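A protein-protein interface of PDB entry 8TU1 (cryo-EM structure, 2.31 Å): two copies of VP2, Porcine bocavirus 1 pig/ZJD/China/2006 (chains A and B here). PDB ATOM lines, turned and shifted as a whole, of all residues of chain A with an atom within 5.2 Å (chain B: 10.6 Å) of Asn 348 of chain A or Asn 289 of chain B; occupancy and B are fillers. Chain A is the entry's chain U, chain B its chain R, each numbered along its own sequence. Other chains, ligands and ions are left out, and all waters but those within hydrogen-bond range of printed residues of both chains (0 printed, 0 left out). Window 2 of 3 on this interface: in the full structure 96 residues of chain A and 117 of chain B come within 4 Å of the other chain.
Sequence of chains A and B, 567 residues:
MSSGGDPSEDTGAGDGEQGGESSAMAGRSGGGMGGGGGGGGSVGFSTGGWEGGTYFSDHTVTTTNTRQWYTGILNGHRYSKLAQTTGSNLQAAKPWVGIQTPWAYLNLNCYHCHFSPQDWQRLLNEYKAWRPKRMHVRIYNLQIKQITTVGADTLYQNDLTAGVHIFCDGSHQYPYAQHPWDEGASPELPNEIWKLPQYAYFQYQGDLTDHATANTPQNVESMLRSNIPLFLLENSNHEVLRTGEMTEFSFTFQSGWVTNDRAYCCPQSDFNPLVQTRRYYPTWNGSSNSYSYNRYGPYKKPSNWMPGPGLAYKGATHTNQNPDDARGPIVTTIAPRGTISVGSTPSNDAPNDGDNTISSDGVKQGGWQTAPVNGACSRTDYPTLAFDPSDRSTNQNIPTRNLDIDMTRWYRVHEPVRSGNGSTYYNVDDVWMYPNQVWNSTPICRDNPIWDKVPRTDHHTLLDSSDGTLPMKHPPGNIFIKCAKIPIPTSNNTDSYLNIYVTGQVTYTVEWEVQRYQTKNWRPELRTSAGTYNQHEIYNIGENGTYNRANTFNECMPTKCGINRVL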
ATOM      1  N   ALA A 214      17.392  -2.420  15.160  1.00  0.00           N
ATOM      2  CA  ALA A 214      18.085  -2.452  16.440  1.00  0.00           C
ATOM      3  C   ALA A 214      19.591  -2.528  16.246  1.00  0.00           C
ATOM      4  O   ALA A 214      20.356  -2.244  17.174  1.00  0.00           O
ATOM      5  CB  ALA A 214      17.597  -3.634  17.273  1.00  0.00           C
ATOM      6  N   ASN A 215      20.030  -2.909  15.055  1.00  0.00           N
ATOM      7  CA  ASN A 215      21.440  -3.075  14.747  1.00  0.00           C
ATOM      8  C   ASN A 215      22.062  -1.857  14.080  1.00  0.00           C
ATOM      9  O   ASN A 215      23.242  -1.909  13.723  1.00  0.00           O
ATOM     10  CB  ASN A 215      21.614  -4.306  13.862  1.00  0.00           C
ATOM     11  CG  ASN A 215      21.333  -5.592  14.607  1.00  0.00           C
ATOM     12  OD1 ASN A 215      21.470  -5.657  15.824  1.00  0.00           O
ATOM     13  ND2 ASN A 215      20.899  -6.611  13.882  1.00  0.00           N
ATOM     14  N   PRO A 346      17.911  -6.940   5.180  1.00  0.00           N
ATOM     15  CA  PRO A 346      18.572  -7.433   6.388  1.00  0.00           C
ATOM     16  C   PRO A 346      18.344  -8.924   6.552  1.00  0.00           C
ATOM     17  O   PRO A 346      17.257  -9.441   6.288  1.00  0.00           O
ATOM     18  CB  PRO A 346      17.908  -6.626   7.507  1.00  0.00           C
ATOM     19  CG  PRO A 346      16.583  -6.276   6.963  1.00  0.00           C
ATOM     20  CD  PRO A 346      16.780  -6.056   5.494  1.00  0.00           C
ATOM     21  N   SER A 347      19.394  -9.619   6.972  1.00  0.00           N
ATOM     22  CA  SER A 347      19.351 -11.058   7.188  1.00  0.00           C
ATOM     23  C   SER A 347      19.704 -11.337   8.639  1.00  0.00           C
ATOM     24  O   SER A 347      20.778 -10.945   9.106  1.00  0.00           O
ATOM     25  CB  SER A 347      20.312 -11.786   6.248  1.00  0.00           C
ATOM     26  OG  SER A 347      20.302 -13.176   6.499  1.00  0.00           O
ATOM     27  N   ASN A 348      18.802 -12.007   9.345  1.00  0.00           N
ATOM     28  CA  ASN A 348      18.992 -12.321  10.752  1.00  0.00           C
ATOM     29  C   ASN A 348      19.574 -13.704  10.980  1.00  0.00           C
ATOM     30  O   ASN A 348      19.814 -14.077  12.129  1.00  0.00           O
ATOM     31  CB  ASN A 348      17.666 -12.180  11.492  1.00  0.00           C
ATOM     32  CG  ASN A 348      17.241 -10.742  11.628  1.00  0.00           C
ATOM     33  OD1 ASN A 348      18.075  -9.843  11.637  1.00  0.00           O
ATOM     34  ND2 ASN A 348      15.941 -10.511  11.686  1.00  0.00           N
ATOM     35  N   ASP A 349      19.813 -14.470   9.926  1.00  0.00           N
ATOM     36  CA  ASP A 349      20.405 -15.790  10.070  1.00  0.00           C
ATOM     37  C   ASP A 349      21.915 -15.721   9.892  1.00  0.00           C
ATOM     38  O   ASP A 349      22.429 -14.925   9.103  1.00  0.00           O
ATOM     39  CB  ASP A 349      19.781 -16.779   9.083  1.00  0.00           C
ATOM     40  CG  ASP A 349      19.893 -16.328   7.651  1.00  0.00           C
ATOM     41  OD1 ASP A 349      20.332 -15.186   7.414  1.00  0.00           O
ATOM     42  OD2 ASP A 349      19.538 -17.118   6.753  1.00  0.00           O
ATOM     43  N   ALA A 350      22.618 -16.536  10.665  1.00  0.00           N
ATOM     44  CA  ALA A 350      24.072 -16.537  10.679  1.00  0.00           C
ATOM     45  C   ALA A 350      24.634 -16.855   9.305  1.00  0.00           C
ATOM     46  O   ALA A 350      24.000 -17.555   8.523  1.00  0.00           O
ATOM     47  CB  ALA A 350      24.571 -17.532  11.696  1.00  0.00           C
ATOM     48  N   ASP A 353      23.615 -12.015  10.747  1.00  0.00           N
ATOM     49  CA  ASP A 353      23.192 -11.504  12.051  1.00  0.00           C
ATOM     50  C   ASP A 353      22.887 -10.004  12.000  1.00  0.00           C
ATOM     51  O   ASP A 353      23.561  -9.175  12.604  1.00  0.00           O
ATOM     52  CB  ASP A 353      24.250 -11.825  13.115  1.00  0.00           C
ATOM     53  CG  ASP A 353      24.306 -13.306  13.457  1.00  0.00           C
ATOM     54  OD1 ASP A 353      23.365 -14.043  13.096  1.00  0.00           O
ATOM     55  OD2 ASP A 353      25.282 -13.739  14.098  1.00  0.00           O
ATOM     56  N   GLY A 354      21.828  -9.678  11.267  1.00  0.00           N
ATOM     57  CA  GLY A 354      21.408  -8.305  11.122  1.00  0.00           C
ATOM     58  C   GLY A 354      22.082  -7.538  10.010  1.00  0.00           C
ATOM     59  O   GLY A 354      21.652  -6.420   9.706  1.00  0.00           O
ATOM     60  N   THR B 283      26.996 -10.614  22.045  1.00  0.00           N
ATOM     61  CA  THR B 283      26.329 -11.908  22.046  1.00  0.00           C
ATOM     62  C   THR B 283      25.047 -11.744  21.252  1.00  0.00           C
ATOM     63  O   THR B 283      24.246 -10.853  21.540  1.00  0.00           O
ATOM     64  CB  THR B 283      26.031 -12.402  23.457  1.00  0.00           C
ATOM     65  OG1 THR B 283      27.254 -12.545  24.179  1.00  0.00           O
ATOM     66  CG2 THR B 283      25.337 -13.738  23.400  1.00  0.00           C
ATOM     67  N   TRP B 284      24.861 -12.593  20.256  1.00  0.00           N
ATOM     68  CA  TRP B 284      23.678 -12.514  19.423  1.00  0.00           C
ATOM     69  C   TRP B 284      22.487 -13.143  20.128  1.00  0.00           C
ATOM     70  O   TRP B 284      22.575 -14.242  20.674  1.00  0.00           O
ATOM     71  CB  TRP B 284      23.932 -13.212  18.094  1.00  0.00           C
ATOM     72  CG  TRP B 284      22.767 -13.216  17.181  1.00  0.00           C
ATOM     73  CD1 TRP B 284      21.959 -14.266  16.897  1.00  0.00           C
ATOM     74  CD2 TRP B 284      22.274 -12.112  16.427  1.00  0.00           C
ATOM     75  NE1 TRP B 284      20.994 -13.892  16.006  1.00  0.00           N
ATOM     76  CE2 TRP B 284      21.165 -12.570  15.700  1.00  0.00           C
ATOM     77  CE3 TRP B 284      22.663 -10.777  16.295  1.00  0.00           C
ATOM     78  CZ2 TRP B 284      20.442 -11.744  14.852  1.00  0.00           C
ATOM     79  CZ3 TRP B 284      21.944  -9.961  15.456  1.00  0.00           C
ATOM     80  CH2 TRP B 284      20.846 -10.446  14.742  1.00  0.00           C
ATOM     81  N   ASN B 285      21.373 -12.432  20.122  1.00  0.00           N
ATOM     82  CA  ASN B 285      20.113 -12.952  20.624  1.00  0.00           C
ATOM     83  C   ASN B 285      19.221 -13.245  19.429  1.00  0.00           C
ATOM     84  O   ASN B 285      18.778 -12.323  18.741  1.00  0.00           O
ATOM     85  CB  ASN B 285      19.451 -11.962  21.575  1.00  0.00           C
ATOM     86  CG  ASN B 285      18.284 -12.565  22.313  1.00  0.00           C
ATOM     87  OD1 ASN B 285      18.258 -13.764  22.580  1.00  0.00           O
ATOM     88  ND2 ASN B 285      17.309 -11.735  22.650  1.00  0.00           N
ATOM     89  N   GLY B 286      18.971 -14.529  19.181  1.00  0.00           N
ATOM     90  CA  GLY B 286      18.166 -14.899  18.029  1.00  0.00           C
ATOM     91  C   GLY B 286      16.720 -14.465  18.160  1.00  0.00           C
ATOM     92  O   GLY B 286      16.028 -14.274  17.159  1.00  0.00           O
ATOM     93  N   SER B 287      16.242 -14.306  19.396  1.00  0.00           N
ATOM     94  CA  SER B 287      14.861 -13.884  19.591  1.00  0.00           C
ATOM     95  C   SER B 287      14.675 -12.418  19.232  1.00  0.00           C
ATOM     96  O   SER B 287      13.785 -12.074  18.447  1.00  0.00           O
ATOM     97  CB  SER B 287      14.432 -14.141  21.033  1.00  0.00           C
ATOM     98  OG  SER B 287      14.422 -15.529  21.311  1.00  0.00           O
ATOM     99  N   SER B 288      15.507 -11.541  19.781  1.00  0.00           N
ATOM    100  CA  SER B 288      15.394 -10.117  19.507  1.00  0.00           C
ATOM    101  C   SER B 288      16.125  -9.697  18.244  1.00  0.00           C
ATOM    102  O   SER B 288      15.981  -8.547  17.822  1.00  0.00           O
ATOM    103  CB  SER B 288      15.927  -9.303  20.685  1.00  0.00           C
ATOM    104  OG  SER B 288      17.315  -9.510  20.859  1.00  0.00           O
ATOM    105  N   ASN B 289      16.906 -10.593  17.644  1.00  0.00           N
ATOM    106  CA  ASN B 289      17.676 -10.294  16.442  1.00  0.00           C
ATOM    107  C   ASN B 289      18.568  -9.078  16.662  1.00  0.00           C
ATOM    108  O   ASN B 289      18.647  -8.170  15.837  1.00  0.00           O
ATOM    109  CB  ASN B 289      16.750 -10.102  15.243  1.00  0.00           C
ATOM    110  CG  ASN B 289      16.106 -11.392  14.804  1.00  0.00           C
ATOM    111  OD1 ASN B 289      16.653 -12.470  15.014  1.00  0.00           O
ATOM    112  ND2 ASN B 289      14.915 -11.296  14.240  1.00  0.00           N
ATOM    113  N   SER B 290      19.245  -9.069  17.803  1.00  0.00           N
ATOM    114  CA  SER B 290      20.114  -7.966  18.175  1.00  0.00           C
ATOM    115  C   SER B 290      21.249  -8.509  19.028  1.00  0.00           C
ATOM    116  O   SER B 290      21.317  -9.703  19.324  1.00  0.00           O
ATOM    117  CB  SER B 290      19.333  -6.878  18.913  1.00  0.00           C
ATOM    118  OG  SER B 290      18.810  -7.364  20.133  1.00  0.00           O
ATOM    119  N   TYR B 291      22.140  -7.619  19.436  1.00  0.00           N
ATOM    120  CA  TYR B 291      23.269  -7.984  20.272  1.00  0.00           C
ATOM    121  C   TYR B 291      23.112  -7.423  21.676  1.00  0.00           C
ATOM    122  O   TYR B 291      22.526  -6.359  21.874  1.00  0.00           O
ATOM    123  CB  TYR B 291      24.586  -7.488  19.685  1.00  0.00           C
ATOM    124  CG  TYR B 291      25.004  -8.174  18.417  1.00  0.00           C
ATOM    125  CD1 TYR B 291      25.703  -9.366  18.462  1.00  0.00           C
ATOM    126  CD2 TYR B 291      24.743  -7.613  17.181  1.00  0.00           C
ATOM    127  CE1 TYR B 291      26.107  -9.993  17.320  1.00  0.00           C
ATOM    128  CE2 TYR B 291      25.141  -8.236  16.028  1.00  0.00           C
ATOM    129  CZ  TYR B 291      25.826  -9.426  16.104  1.00  0.00           C
ATOM    130  OH  TYR B 291      26.237 -10.060  14.964  1.00  0.00           O
ATOM    131  N   SER B 292      23.651  -8.156  22.638  1.00  0.00           N
ATOM    132  CA  SER B 292      23.857  -7.698  23.998  1.00  0.00           C
ATOM    133  C   SER B 292      25.346  -7.776  24.285  1.00  0.00           C
ATOM    134  O   SER B 292      26.094  -8.433  23.557  1.00  0.00           O
ATOM    135  CB  SER B 292      23.072  -8.541  24.999  1.00  0.00           C
ATOM    136  OG  SER B 292      23.530  -9.878  24.999  1.00  0.00           O
ATOM    137  N   TYR B 293      25.791  -7.079  25.319  1.00  0.00           N
ATOM    138  CA  TYR B 293      27.216  -6.919  25.554  1.00  0.00           C
ATOM    139  C   TYR B 293      27.599  -7.330  26.963  1.00  0.00           C
ATOM    140  O   TYR B 293      26.824  -7.168  27.906  1.00  0.00           O
ATOM    141  CB  TYR B 293      27.643  -5.489  25.293  1.00  0.00           C
ATOM    142  CG  TYR B 293      27.437  -5.091  23.864  1.00  0.00           C
ATOM    143  CD1 TYR B 293      28.397  -5.359  22.905  1.00  0.00           C
ATOM    144  CD2 TYR B 293      26.272  -4.462  23.467  1.00  0.00           C
ATOM    145  CE1 TYR B 293      28.204  -5.000  21.599  1.00  0.00           C
ATOM    146  CE2 TYR B 293      26.075  -4.102  22.169  1.00  0.00           C
ATOM    147  CZ  TYR B 293      27.042  -4.369  21.239  1.00  0.00           C
ATOM    148  OH  TYR B 293      26.834  -4.004  19.938  1.00  0.00           O
ATOM    149  N   ARG B 418      29.350 -17.789  14.255  1.00  0.00           N
ATOM    150  CA  ARG B 418      28.137 -18.284  14.881  1.00  0.00           C
ATOM    151  C   ARG B 418      27.395 -19.163  13.891  1.00  0.00           C
ATOM    152  O   ARG B 418      27.153 -18.765  12.752  1.00  0.00           O
ATOM    153  CB  ARG B 418      27.238 -17.136  15.326  1.00  0.00           C
ATOM    154  CG  ARG B 418      26.056 -17.617  16.150  1.00  0.00           C
ATOM    155  CD  ARG B 418      25.121 -16.506  16.578  1.00  0.00           C
ATOM    156  NE  ARG B 418      24.363 -15.974  15.458  1.00  0.00           N
ATOM    157  CZ  ARG B 418      23.248 -16.527  15.000  1.00  0.00           C
ATOM    158  NH1 ARG B 418      22.769 -17.620  15.574  1.00  0.00           N
ATOM    159  NH2 ARG B 418      22.605 -15.989  13.981  1.00  0.00           N
ATOM    160  N   SER B 419      27.077 -20.381  14.311  1.00  0.00           N
ATOM    161  CA  SER B 419      26.366 -21.319  13.460  1.00  0.00           C
ATOM    162  C   SER B 419      25.291 -22.001  14.285  1.00  0.00           C
ATOM    163  O   SER B 419      25.606 -22.718  15.237  1.00  0.00           O
ATOM    164  CB  SER B 419      27.328 -22.349  12.866  1.00  0.00           C
ATOM    165  OG  SER B 419      27.914 -23.126  13.892  1.00  0.00           O
ATOM    166  N   GLY B 420      24.036 -21.806  13.901  1.00  0.00           N
ATOM    167  CA  GLY B 420      22.948 -22.430  14.633  1.00  0.00           C
ATOM    168  C   GLY B 420      22.971 -22.044  16.097  1.00  0.00           C
ATOM    169  O   GLY B 420      22.991 -20.862  16.456  1.00  0.00           O
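No position is printed for both chains. Of the 11 pairs that touch across the chains among the printed residues, none has its exchanged pair printed and touching as well.
The guanidinium group of Arg 418 of chain B is in salt-bridge range of the side-chain carboxylate of Asp 353 of chain A, 2.8 Å away. The side-chain amide nitrogen (ND2) of Asn 289 of chain B sits close to the side-chain amide nitrogen (ND2) of Asn 348 of chain A (2.9 Å). O of Asn 289 of chain B lies within hydrogen-bond range of ND2 of Asn 215 of chain A. The backbone NH (N) of Ala 350 of chain A sits close to the guanidinium group (NH2) of Arg 418 of chain B (3.4 Å).
N of Asp 353 of chain A is in hydrogen-bond range of O of Ser 347 of chain A (3.4 Å). The side-chain hydroxyl of Ser 288 of chain B lies within hydrogen-bond range of the side-chain hydroxyl of Ser 290 of chain B (2.7 Å). O of Gly 286 of chain B lies close to OD1 of Asn 289 of chain B, at 2.9 Å. O of Ser 290 of chain B is in hydrogen-bond range of N of Asn 285 of chain B. O of Ser 347 of chain A lies within hydrogen-bond range of N of Gly 354 of chain A, 2.7 Å away. The backbone carbonyl oxygen (O) of Gly 420 of chain B lies within hydrogen-bond range of the guanidinium group (NH1) of Arg 418 of chain B (3.4 Å).
Of the 9 printed residues of chain A, 5 touch a printed residue of chain B. Along chain B the printed residues that touch a printed residue of chain A span positions 284 to 418.
No residue of chain B comes within 4 Å of Ala 214 of chain A. Of the printed residues of chain B, Asn 215 of chain A touches Trp 284, Asn 289 and Ser 290. Ser 347 of chain A touches none of the printed residues of chain B. Asn 348 of chain A touches three residues of chain B. No residue of chain B comes within 4 Å of Asp 349 of chain A. Of chain B, only Arg 418 (3.0 Å) comes within 4 Å of Ala 350 of chain A. Asp 353 of chain A touches just these residues of chain B: Trp 284, Tyr 291 and Arg 418. Thr 283 of chain B touches none of the printed residues of chain A. Of the printed residues of chain A, Trp 284 of chain B touches Asn 215, Asn 348, Asp 353 and Gly 354. Asn 289 of chain B touches just these residues of chain A: Asn 215 and Asn 348. Printed residues of chain A within 4 Å of Tyr 291 of chain B: Asp 353 (3.2 Å). Of the printed residues of chain A, Arg 418 of chain B touches Asn 348 (3.9 Å), Ala 350 (3.0 Å) and Asp 353 (2.3 Å). The nearest residue of chain B that does not touch Asn 348 of chain A is Gly 286 of chain B (6.2 Å). The nearest printed residue of chain A that does not touch Arg 418 of chain B is Asp 349 of chain A (4.2 Å).
Among the printed residues, merely in contact across the chains: Asn 215 of chain A with Trp 284 of chain B (3.8 Å), Asn 215 of chain A with Ser 290 of chain B (3.6 Å), Asn 348 of chain A with Trp 284 of chain B (3.6 Å), Asn 348 of chain A with Arg 418 of chain B (3.9 Å), Asp 353 of chain A with Trp 284 of chain B (3.4 Å), Asp 353 of chain A with Tyr 291 of chain B (3.2 Å) and Gly 354 of chain A with Trp 284 of chain B (3.7 Å).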
